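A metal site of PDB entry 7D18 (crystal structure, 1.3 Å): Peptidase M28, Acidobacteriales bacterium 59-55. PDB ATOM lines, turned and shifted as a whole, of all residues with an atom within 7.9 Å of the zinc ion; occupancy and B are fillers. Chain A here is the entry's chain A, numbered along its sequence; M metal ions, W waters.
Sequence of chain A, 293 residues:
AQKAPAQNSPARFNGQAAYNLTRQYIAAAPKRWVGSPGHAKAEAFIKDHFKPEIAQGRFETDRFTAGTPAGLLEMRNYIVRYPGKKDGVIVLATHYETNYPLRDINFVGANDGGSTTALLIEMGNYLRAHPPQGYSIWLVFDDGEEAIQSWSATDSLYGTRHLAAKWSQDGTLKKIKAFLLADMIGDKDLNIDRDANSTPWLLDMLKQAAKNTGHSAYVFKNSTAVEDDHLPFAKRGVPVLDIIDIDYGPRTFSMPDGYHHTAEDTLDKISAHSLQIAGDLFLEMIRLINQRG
Water W1 bridges a ring nitrogen (NE2) of His 260 (2.6 Å) and the side-chain carboxylate of Asp 112 (3.5 Å).
OE2 of Glu 146 binds the zinc ion, 1.9 Å away. Water W1 is bound to the zinc ion, at 1.9 Å. The side-chain carboxylate (OD2) of Asp 112 binds the zinc ion, at 2.0 Å. The zinc ion is bound by NE2 of His 261 (2.0 Å).
Merely in contact with the zinc ion: His 260 (3.6 Å). Within 4 Å of the zinc ion: Asp 112, Glu 146, His 260 and His 261. The nearest printed residue that does not touch the zinc ion is Asn 99 (4.1 Å).
The side-chain carboxylate (OE1) of Glu 146 lies within hydrogen-bond range of the side-chain amide nitrogen (ND2) of Asn 99. N of Glu 146 is in hydrogen-bond range of OE2 of Glu 97 (2.9 Å). The side-chain carboxylate (OD1) of Asp 112 is in hydrogen-bond range of a ring nitrogen (NE2) of His 95 (2.8 Å). N of Asp 112 sits close to OD2 of Asp 265 (3.3 Å). A ring nitrogen (NE2) of His 260 lies close to a ring nitrogen (NE2) of His 261 (3.4 Å). NE2 of His 261 lies close to ND2 of Asn 99, 3.4 Å away. A ring nitrogen (NE2) of His 260 is in hydrogen-bond range of the side-chain sulfur of Met 184 (3.7 Å).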
ATOM      1  N   HIS A  95     -10.844 -21.841 -26.835  1.00  0.00           N
ATOM      2  CA  HIS A  95     -11.065 -20.611 -26.091  1.00  0.00           C
ATOM      3  C   HIS A  95     -11.370 -20.965 -24.645  1.00  0.00           C
ATOM      4  O   HIS A  95     -11.778 -22.087 -24.338  1.00  0.00           O
ATOM      5  CB  HIS A  95     -12.153 -19.711 -26.724  1.00  0.00           C
ATOM      6  CG  HIS A  95     -13.560 -20.016 -26.295  1.00  0.00           C
ATOM      7  ND1 HIS A  95     -14.283 -19.180 -25.463  1.00  0.00           N
ATOM      8  CD2 HIS A  95     -14.421 -21.017 -26.631  1.00  0.00           C
ATOM      9  CE1 HIS A  95     -15.506 -19.646 -25.304  1.00  0.00           C
ATOM     10  NE2 HIS A  95     -15.627 -20.750 -26.005  1.00  0.00           N
ATOM     11  N   GLU A  97     -12.643 -18.224 -22.143  1.00  0.00           N
ATOM     12  CA  GLU A  97     -13.407 -17.181 -21.463  1.00  0.00           C
ATOM     13  C   GLU A  97     -14.904 -17.359 -21.756  1.00  0.00           C
ATOM     14  O   GLU A  97     -15.294 -18.094 -22.660  1.00  0.00           O
ATOM     15  CB  GLU A  97     -12.899 -15.793 -21.926  1.00  0.00           C
ATOM     16  CG  GLU A  97     -13.649 -15.102 -23.069  1.00  0.00           C
ATOM     17  CD  GLU A  97     -13.643 -15.847 -24.408  1.00  0.00           C
ATOM     18  OE1 GLU A  97     -12.961 -16.890 -24.603  1.00  0.00           O
ATOM     19  OE2 GLU A  97     -14.349 -15.365 -25.318  1.00  0.00           O
ATOM     20  N   THR A  98     -15.741 -16.639 -20.997  1.00  0.00           N
ATOM     21  CA  THR A  98     -17.188 -16.662 -21.237  1.00  0.00           C
ATOM     22  C   THR A  98     -17.667 -15.321 -21.780  1.00  0.00           C
ATOM     23  O   THR A  98     -16.991 -14.279 -21.662  1.00  0.00           O
ATOM     24  CB  THR A  98     -17.969 -17.016 -19.970  1.00  0.00           C
ATOM     25  OG1 THR A  98     -17.633 -16.110 -18.917  1.00  0.00           O
ATOM     26  CG2 THR A  98     -17.693 -18.452 -19.516  1.00  0.00           C
ATOM     27  N   ASN A  99     -18.890 -15.327 -22.316  1.00  0.00           N
ATOM     28  CA  ASN A  99     -19.434 -14.193 -23.059  1.00  0.00           C
ATOM     29  C   ASN A  99     -19.690 -12.974 -22.174  1.00  0.00           C
ATOM     30  O   ASN A  99     -20.455 -13.050 -21.204  1.00  0.00           O
ATOM     31  CB  ASN A  99     -20.769 -14.587 -23.679  1.00  0.00           C
ATOM     32  CG  ASN A  99     -20.679 -15.766 -24.596  1.00  0.00           C
ATOM     33  OD1 ASN A  99     -20.180 -16.833 -24.228  1.00  0.00           O
ATOM     34  ND2 ASN A  99     -21.159 -15.603 -25.808  1.00  0.00           N
ATOM     35  N   LEU A 102     -23.326 -11.991 -21.388  1.00  0.00           N
ATOM     36  CA  LEU A 102     -23.997 -12.911 -20.479  1.00  0.00           C
ATOM     37  C   LEU A 102     -23.485 -12.770 -19.051  1.00  0.00           C
ATOM     38  O   LEU A 102     -23.747 -13.653 -18.213  1.00  0.00           O
ATOM     39  CB  LEU A 102     -23.876 -14.358 -20.971  1.00  0.00           C
ATOM     40  CG  LEU A 102     -24.311 -14.580 -22.421  1.00  0.00           C
ATOM     41  CD1 LEU A 102     -24.128 -16.043 -22.823  1.00  0.00           C
ATOM     42  CD2 LEU A 102     -25.755 -14.126 -22.637  1.00  0.00           C
ATOM     43  N   PHE A 107     -24.280 -17.911 -16.533  1.00  0.00           N
ATOM     44  CA  PHE A 107     -23.664 -18.582 -17.674  1.00  0.00           C
ATOM     45  C   PHE A 107     -22.225 -18.929 -17.304  1.00  0.00           C
ATOM     46  O   PHE A 107     -21.407 -18.037 -17.040  1.00  0.00           O
ATOM     47  CB  PHE A 107     -23.675 -17.707 -18.919  1.00  0.00           C
ATOM     48  CG  PHE A 107     -22.984 -18.353 -20.084  1.00  0.00           C
ATOM     49  CD1 PHE A 107     -23.585 -19.422 -20.737  1.00  0.00           C
ATOM     50  CD2 PHE A 107     -21.723 -17.963 -20.491  1.00  0.00           C
ATOM     51  CE1 PHE A 107     -22.970 -20.057 -21.816  1.00  0.00           C
ATOM     52  CE2 PHE A 107     -21.079 -18.610 -21.542  1.00  0.00           C
ATOM     53  CZ  PHE A 107     -21.696 -19.654 -22.198  1.00  0.00           C
ATOM     54  N   GLY A 109     -20.493 -21.567 -19.217  1.00  0.00           N
ATOM     55  CA  GLY A 109     -19.798 -22.136 -20.361  1.00  0.00           C
ATOM     56  C   GLY A 109     -19.192 -23.505 -20.074  1.00  0.00           C
ATOM     57  O   GLY A 109     -18.020 -23.759 -20.375  1.00  0.00           O
ATOM     58  N   ASN A 111     -19.817 -26.508 -21.423  1.00  0.00           N
ATOM     59  CA  ASN A 111     -19.419 -27.124 -22.694  1.00  0.00           C
ATOM     60  C   ASN A 111     -18.624 -26.145 -23.556  1.00  0.00           C
ATOM     61  O   ASN A 111     -17.617 -26.515 -24.169  1.00  0.00           O
ATOM     62  CB  ASN A 111     -20.657 -27.626 -23.446  1.00  0.00           C
ATOM     63  CG  ASN A 111     -20.304 -28.449 -24.660  1.00  0.00           C
ATOM     64  OD1 ASN A 111     -19.280 -29.153 -24.668  1.00  0.00           O
ATOM     65  ND2 ASN A 111     -21.147 -28.366 -25.708  1.00  0.00           N
ATOM     66  N   ASP A 112     -19.052 -24.878 -23.549  1.00  0.00           N
ATOM     67  CA  ASP A 112     -18.555 -23.851 -24.461  1.00  0.00           C
ATOM     68  C   ASP A 112     -17.358 -23.152 -23.822  1.00  0.00           C
ATOM     69  O   ASP A 112     -17.504 -22.112 -23.170  1.00  0.00           O
ATOM     70  CB  ASP A 112     -19.698 -22.892 -24.727  1.00  0.00           C
ATOM     71  CG  ASP A 112     -19.364 -21.840 -25.737  1.00  0.00           C
ATOM     72  OD1 ASP A 112     -18.233 -21.810 -26.282  1.00  0.00           O
ATOM     73  OD2 ASP A 112     -20.267 -20.969 -25.962  1.00  0.00           O
ATOM     74  N   GLY A 113     -16.176 -23.717 -24.031  1.00  0.00           N
ATOM     75  CA  GLY A 113     -14.954 -23.209 -23.443  1.00  0.00           C
ATOM     76  C   GLY A 113     -14.464 -24.053 -22.290  1.00  0.00           C
ATOM     77  O   GLY A 113     -13.289 -24.436 -22.232  1.00  0.00           O
ATOM     78  N   GLU A 145     -12.641 -15.063 -27.734  1.00  0.00           N
ATOM     79  CA  GLU A 145     -13.271 -15.647 -28.920  1.00  0.00           C
ATOM     80  C   GLU A 145     -14.687 -15.107 -29.081  1.00  0.00           C
ATOM     81  O   GLU A 145     -15.117 -14.798 -30.202  1.00  0.00           O
ATOM     82  CB  GLU A 145     -13.299 -17.171 -28.791  1.00  0.00           C
ATOM     83  CG  GLU A 145     -13.927 -17.853 -30.002  1.00  0.00           C
ATOM     84  CD  GLU A 145     -15.362 -18.274 -29.750  1.00  0.00           C
ATOM     85  OE1 GLU A 145     -15.707 -18.610 -28.578  1.00  0.00           O
ATOM     86  OE2 GLU A 145     -16.139 -18.300 -30.713  1.00  0.00           O
ATOM     87  N   GLU A 146     -15.427 -15.010 -27.992  1.00  0.00           N
ATOM     88  CA  GLU A 146     -16.822 -14.606 -28.056  1.00  0.00           C
ATOM     89  C   GLU A 146     -16.944 -13.099 -28.293  1.00  0.00           C
ATOM     90  O   GLU A 146     -16.098 -12.318 -27.872  1.00  0.00           O
ATOM     91  CB  GLU A 146     -17.534 -14.980 -26.762  1.00  0.00           C
ATOM     92  CG  GLU A 146     -17.416 -16.435 -26.366  1.00  0.00           C
ATOM     93  CD  GLU A 146     -18.380 -17.353 -27.094  1.00  0.00           C
ATOM     94  OE1 GLU A 146     -19.077 -16.924 -28.048  1.00  0.00           O
ATOM     95  OE2 GLU A 146     -18.431 -18.550 -26.680  1.00  0.00           O
ATOM     96  N   ALA A 147     -18.001 -12.700 -28.999  1.00  0.00           N
ATOM     97  CA  ALA A 147     -18.241 -11.283 -29.251  1.00  0.00           C
ATOM     98  C   ALA A 147     -18.419 -10.532 -27.931  1.00  0.00           C
ATOM     99  O   ALA A 147     -19.055 -11.025 -26.990  1.00  0.00           O
ATOM    100  CB  ALA A 147     -19.528 -11.128 -30.064  1.00  0.00           C
ATOM    101  N   TRP A 151     -21.929 -10.626 -32.447  1.00  0.00           N
ATOM    102  CA  TRP A 151     -20.993 -11.337 -33.307  1.00  0.00           C
ATOM    103  C   TRP A 151     -20.905 -10.677 -34.682  1.00  0.00           C
ATOM    104  O   TRP A 151     -21.933 -10.418 -35.321  1.00  0.00           O
ATOM    105  CB  TRP A 151     -21.465 -12.779 -33.448  1.00  0.00           C
ATOM    106  CG  TRP A 151     -20.515 -13.672 -34.191  1.00  0.00           C
ATOM    107  CD1 TRP A 151     -20.494 -13.927 -35.523  1.00  0.00           C
ATOM    108  CD2 TRP A 151     -19.461 -14.467 -33.613  1.00  0.00           C
ATOM    109  NE1 TRP A 151     -19.495 -14.822 -35.821  1.00  0.00           N
ATOM    110  CE2 TRP A 151     -18.859 -15.180 -34.661  1.00  0.00           C
ATOM    111  CE3 TRP A 151     -19.003 -14.662 -32.307  1.00  0.00           C
ATOM    112  CZ2 TRP A 151     -17.794 -16.055 -34.456  1.00  0.00           C
ATOM    113  CZ3 TRP A 151     -17.968 -15.532 -32.101  1.00  0.00           C
ATOM    114  CH2 TRP A 151     -17.362 -16.219 -33.173  1.00  0.00           C
ATOM    115  N   ASP A 183     -13.890 -27.402 -29.898  1.00  0.00           N
ATOM    116  CA  ASP A 183     -14.958 -26.470 -29.456  1.00  0.00           C
ATOM    117  C   ASP A 183     -16.250 -27.241 -29.173  1.00  0.00           C
ATOM    118  O   ASP A 183     -16.708 -27.958 -30.061  1.00  0.00           O
ATOM    119  CB  ASP A 183     -15.181 -25.351 -30.482  1.00  0.00           C
ATOM    120  CG  ASP A 183     -15.888 -24.124 -29.938  1.00  0.00           C
ATOM    121  OD1 ASP A 183     -16.211 -24.112 -28.745  1.00  0.00           O
ATOM    122  OD2 ASP A 183     -16.110 -23.177 -30.720  1.00  0.00           O
ATOM    123  N   MET A 184     -16.715 -27.188 -27.918  1.00  0.00           N
ATOM    124  CA  MET A 184     -18.040 -27.704 -27.545  1.00  0.00           C
ATOM    125  C   MET A 184     -18.158 -29.216 -27.672  1.00  0.00           C
ATOM    126  O   MET A 184     -19.229 -29.750 -27.956  1.00  0.00           O
ATOM    127  CB  MET A 184     -19.173 -26.979 -28.277  1.00  0.00           C
ATOM    128  CG  MET A 184     -19.325 -25.534 -27.755  1.00  0.00           C
ATOM    129  SD  MET A 184     -20.354 -24.439 -28.760  1.00  0.00           S
ATOM    130  CE  MET A 184     -21.871 -25.363 -28.850  1.00  0.00           C
ATOM    131  N   ASP A 228     -15.463 -19.460 -36.324  1.00  0.00           N
ATOM    132  CA  ASP A 228     -14.803 -19.823 -35.083  1.00  0.00           C
ATOM    133  C   ASP A 228     -13.336 -19.430 -35.177  1.00  0.00           C
ATOM    134  O   ASP A 228     -12.883 -18.862 -36.192  1.00  0.00           O
ATOM    135  CB  ASP A 228     -14.985 -21.329 -34.836  1.00  0.00           C
ATOM    136  CG  ASP A 228     -14.894 -21.744 -33.363  1.00  0.00           C
ATOM    137  OD1 ASP A 228     -14.468 -20.980 -32.472  1.00  0.00           O
ATOM    138  OD2 ASP A 228     -15.274 -22.929 -33.114  1.00  0.00           O
ATOM    139  N   ILE A 246     -21.594 -28.141 -32.867  1.00  0.00           N
ATOM    140  CA  ILE A 246     -22.334 -26.887 -32.751  1.00  0.00           C
ATOM    141  C   ILE A 246     -23.819 -27.124 -32.522  1.00  0.00           C
ATOM    142  O   ILE A 246     -24.580 -26.172 -32.363  1.00  0.00           O
ATOM    143  CB  ILE A 246     -22.013 -25.977 -33.965  1.00  0.00           C
ATOM    144  CG1 ILE A 246     -22.438 -24.519 -33.731  1.00  0.00           C
ATOM    145  CG2 ILE A 246     -22.686 -26.503 -35.218  1.00  0.00           C
ATOM    146  CD1 ILE A 246     -21.829 -23.888 -32.512  1.00  0.00           C
ATOM    147  N   HIS A 260     -26.877 -23.562 -26.132  1.00  0.00           N
ATOM    148  CA  HIS A 260     -25.792 -22.673 -26.509  1.00  0.00           C
ATOM    149  C   HIS A 260     -26.072 -21.249 -26.055  1.00  0.00           C
ATOM    150  O   HIS A 260     -27.124 -20.680 -26.383  1.00  0.00           O
ATOM    151  CB  HIS A 260     -25.674 -22.738 -28.027  1.00  0.00           C
ATOM    152  CG  HIS A 260     -24.434 -22.130 -28.604  1.00  0.00           C
ATOM    153  ND1 HIS A 260     -24.415 -21.600 -29.880  1.00  0.00           N
ATOM    154  CD2 HIS A 260     -23.155 -22.019 -28.143  1.00  0.00           C
ATOM    155  CE1 HIS A 260     -23.212 -21.160 -30.159  1.00  0.00           C
ATOM    156  NE2 HIS A 260     -22.417 -21.399 -29.122  1.00  0.00           N
ATOM    157  N   HIS A 261     -25.147 -20.681 -25.287  1.00  0.00           N
ATOM    158  CA  HIS A 261     -25.240 -19.300 -24.802  1.00  0.00           C
ATOM    159  C   HIS A 261     -26.433 -19.079 -23.899  1.00  0.00           C
ATOM    160  O   HIS A 261     -26.968 -17.979 -23.823  1.00  0.00           O
ATOM    161  CB  HIS A 261     -25.175 -18.305 -25.963  1.00  0.00           C
ATOM    162  CG  HIS A 261     -23.850 -18.343 -26.661  1.00  0.00           C
ATOM    163  ND1 HIS A 261     -23.646 -17.860 -27.928  1.00  0.00           N
ATOM    164  CD2 HIS A 261     -22.655 -18.815 -26.244  1.00  0.00           C
ATOM    165  CE1 HIS A 261     -22.381 -18.036 -28.270  1.00  0.00           C
ATOM    166  NE2 HIS A 261     -21.752 -18.634 -27.268  1.00  0.00           N
ATOM    167  N   ASP A 265     -26.076 -24.168 -20.068  1.00  0.00           N
ATOM    168  CA  ASP A 265     -24.793 -24.755 -20.457  1.00  0.00           C
ATOM    169  C   ASP A 265     -24.007 -25.048 -19.176  1.00  0.00           C
ATOM    170  O   ASP A 265     -23.118 -24.307 -18.755  1.00  0.00           O
ATOM    171  CB  ASP A 265     -24.044 -23.795 -21.376  1.00  0.00           C
ATOM    172  CG  ASP A 265     -22.693 -24.337 -21.785  1.00  0.00           C
ATOM    173  OD1 ASP A 265     -22.410 -25.524 -21.481  1.00  0.00           O
ATOM    174  OD2 ASP A 265     -21.922 -23.606 -22.454  1.00  0.00           O
HETATM  175 ZN    ZN M   1     -19.922 -19.552 -27.278  1.00  0.00          ZN
HETATM  176  O   HOH W   1     -19.945 -20.488 -28.980  1.00  0.00           O
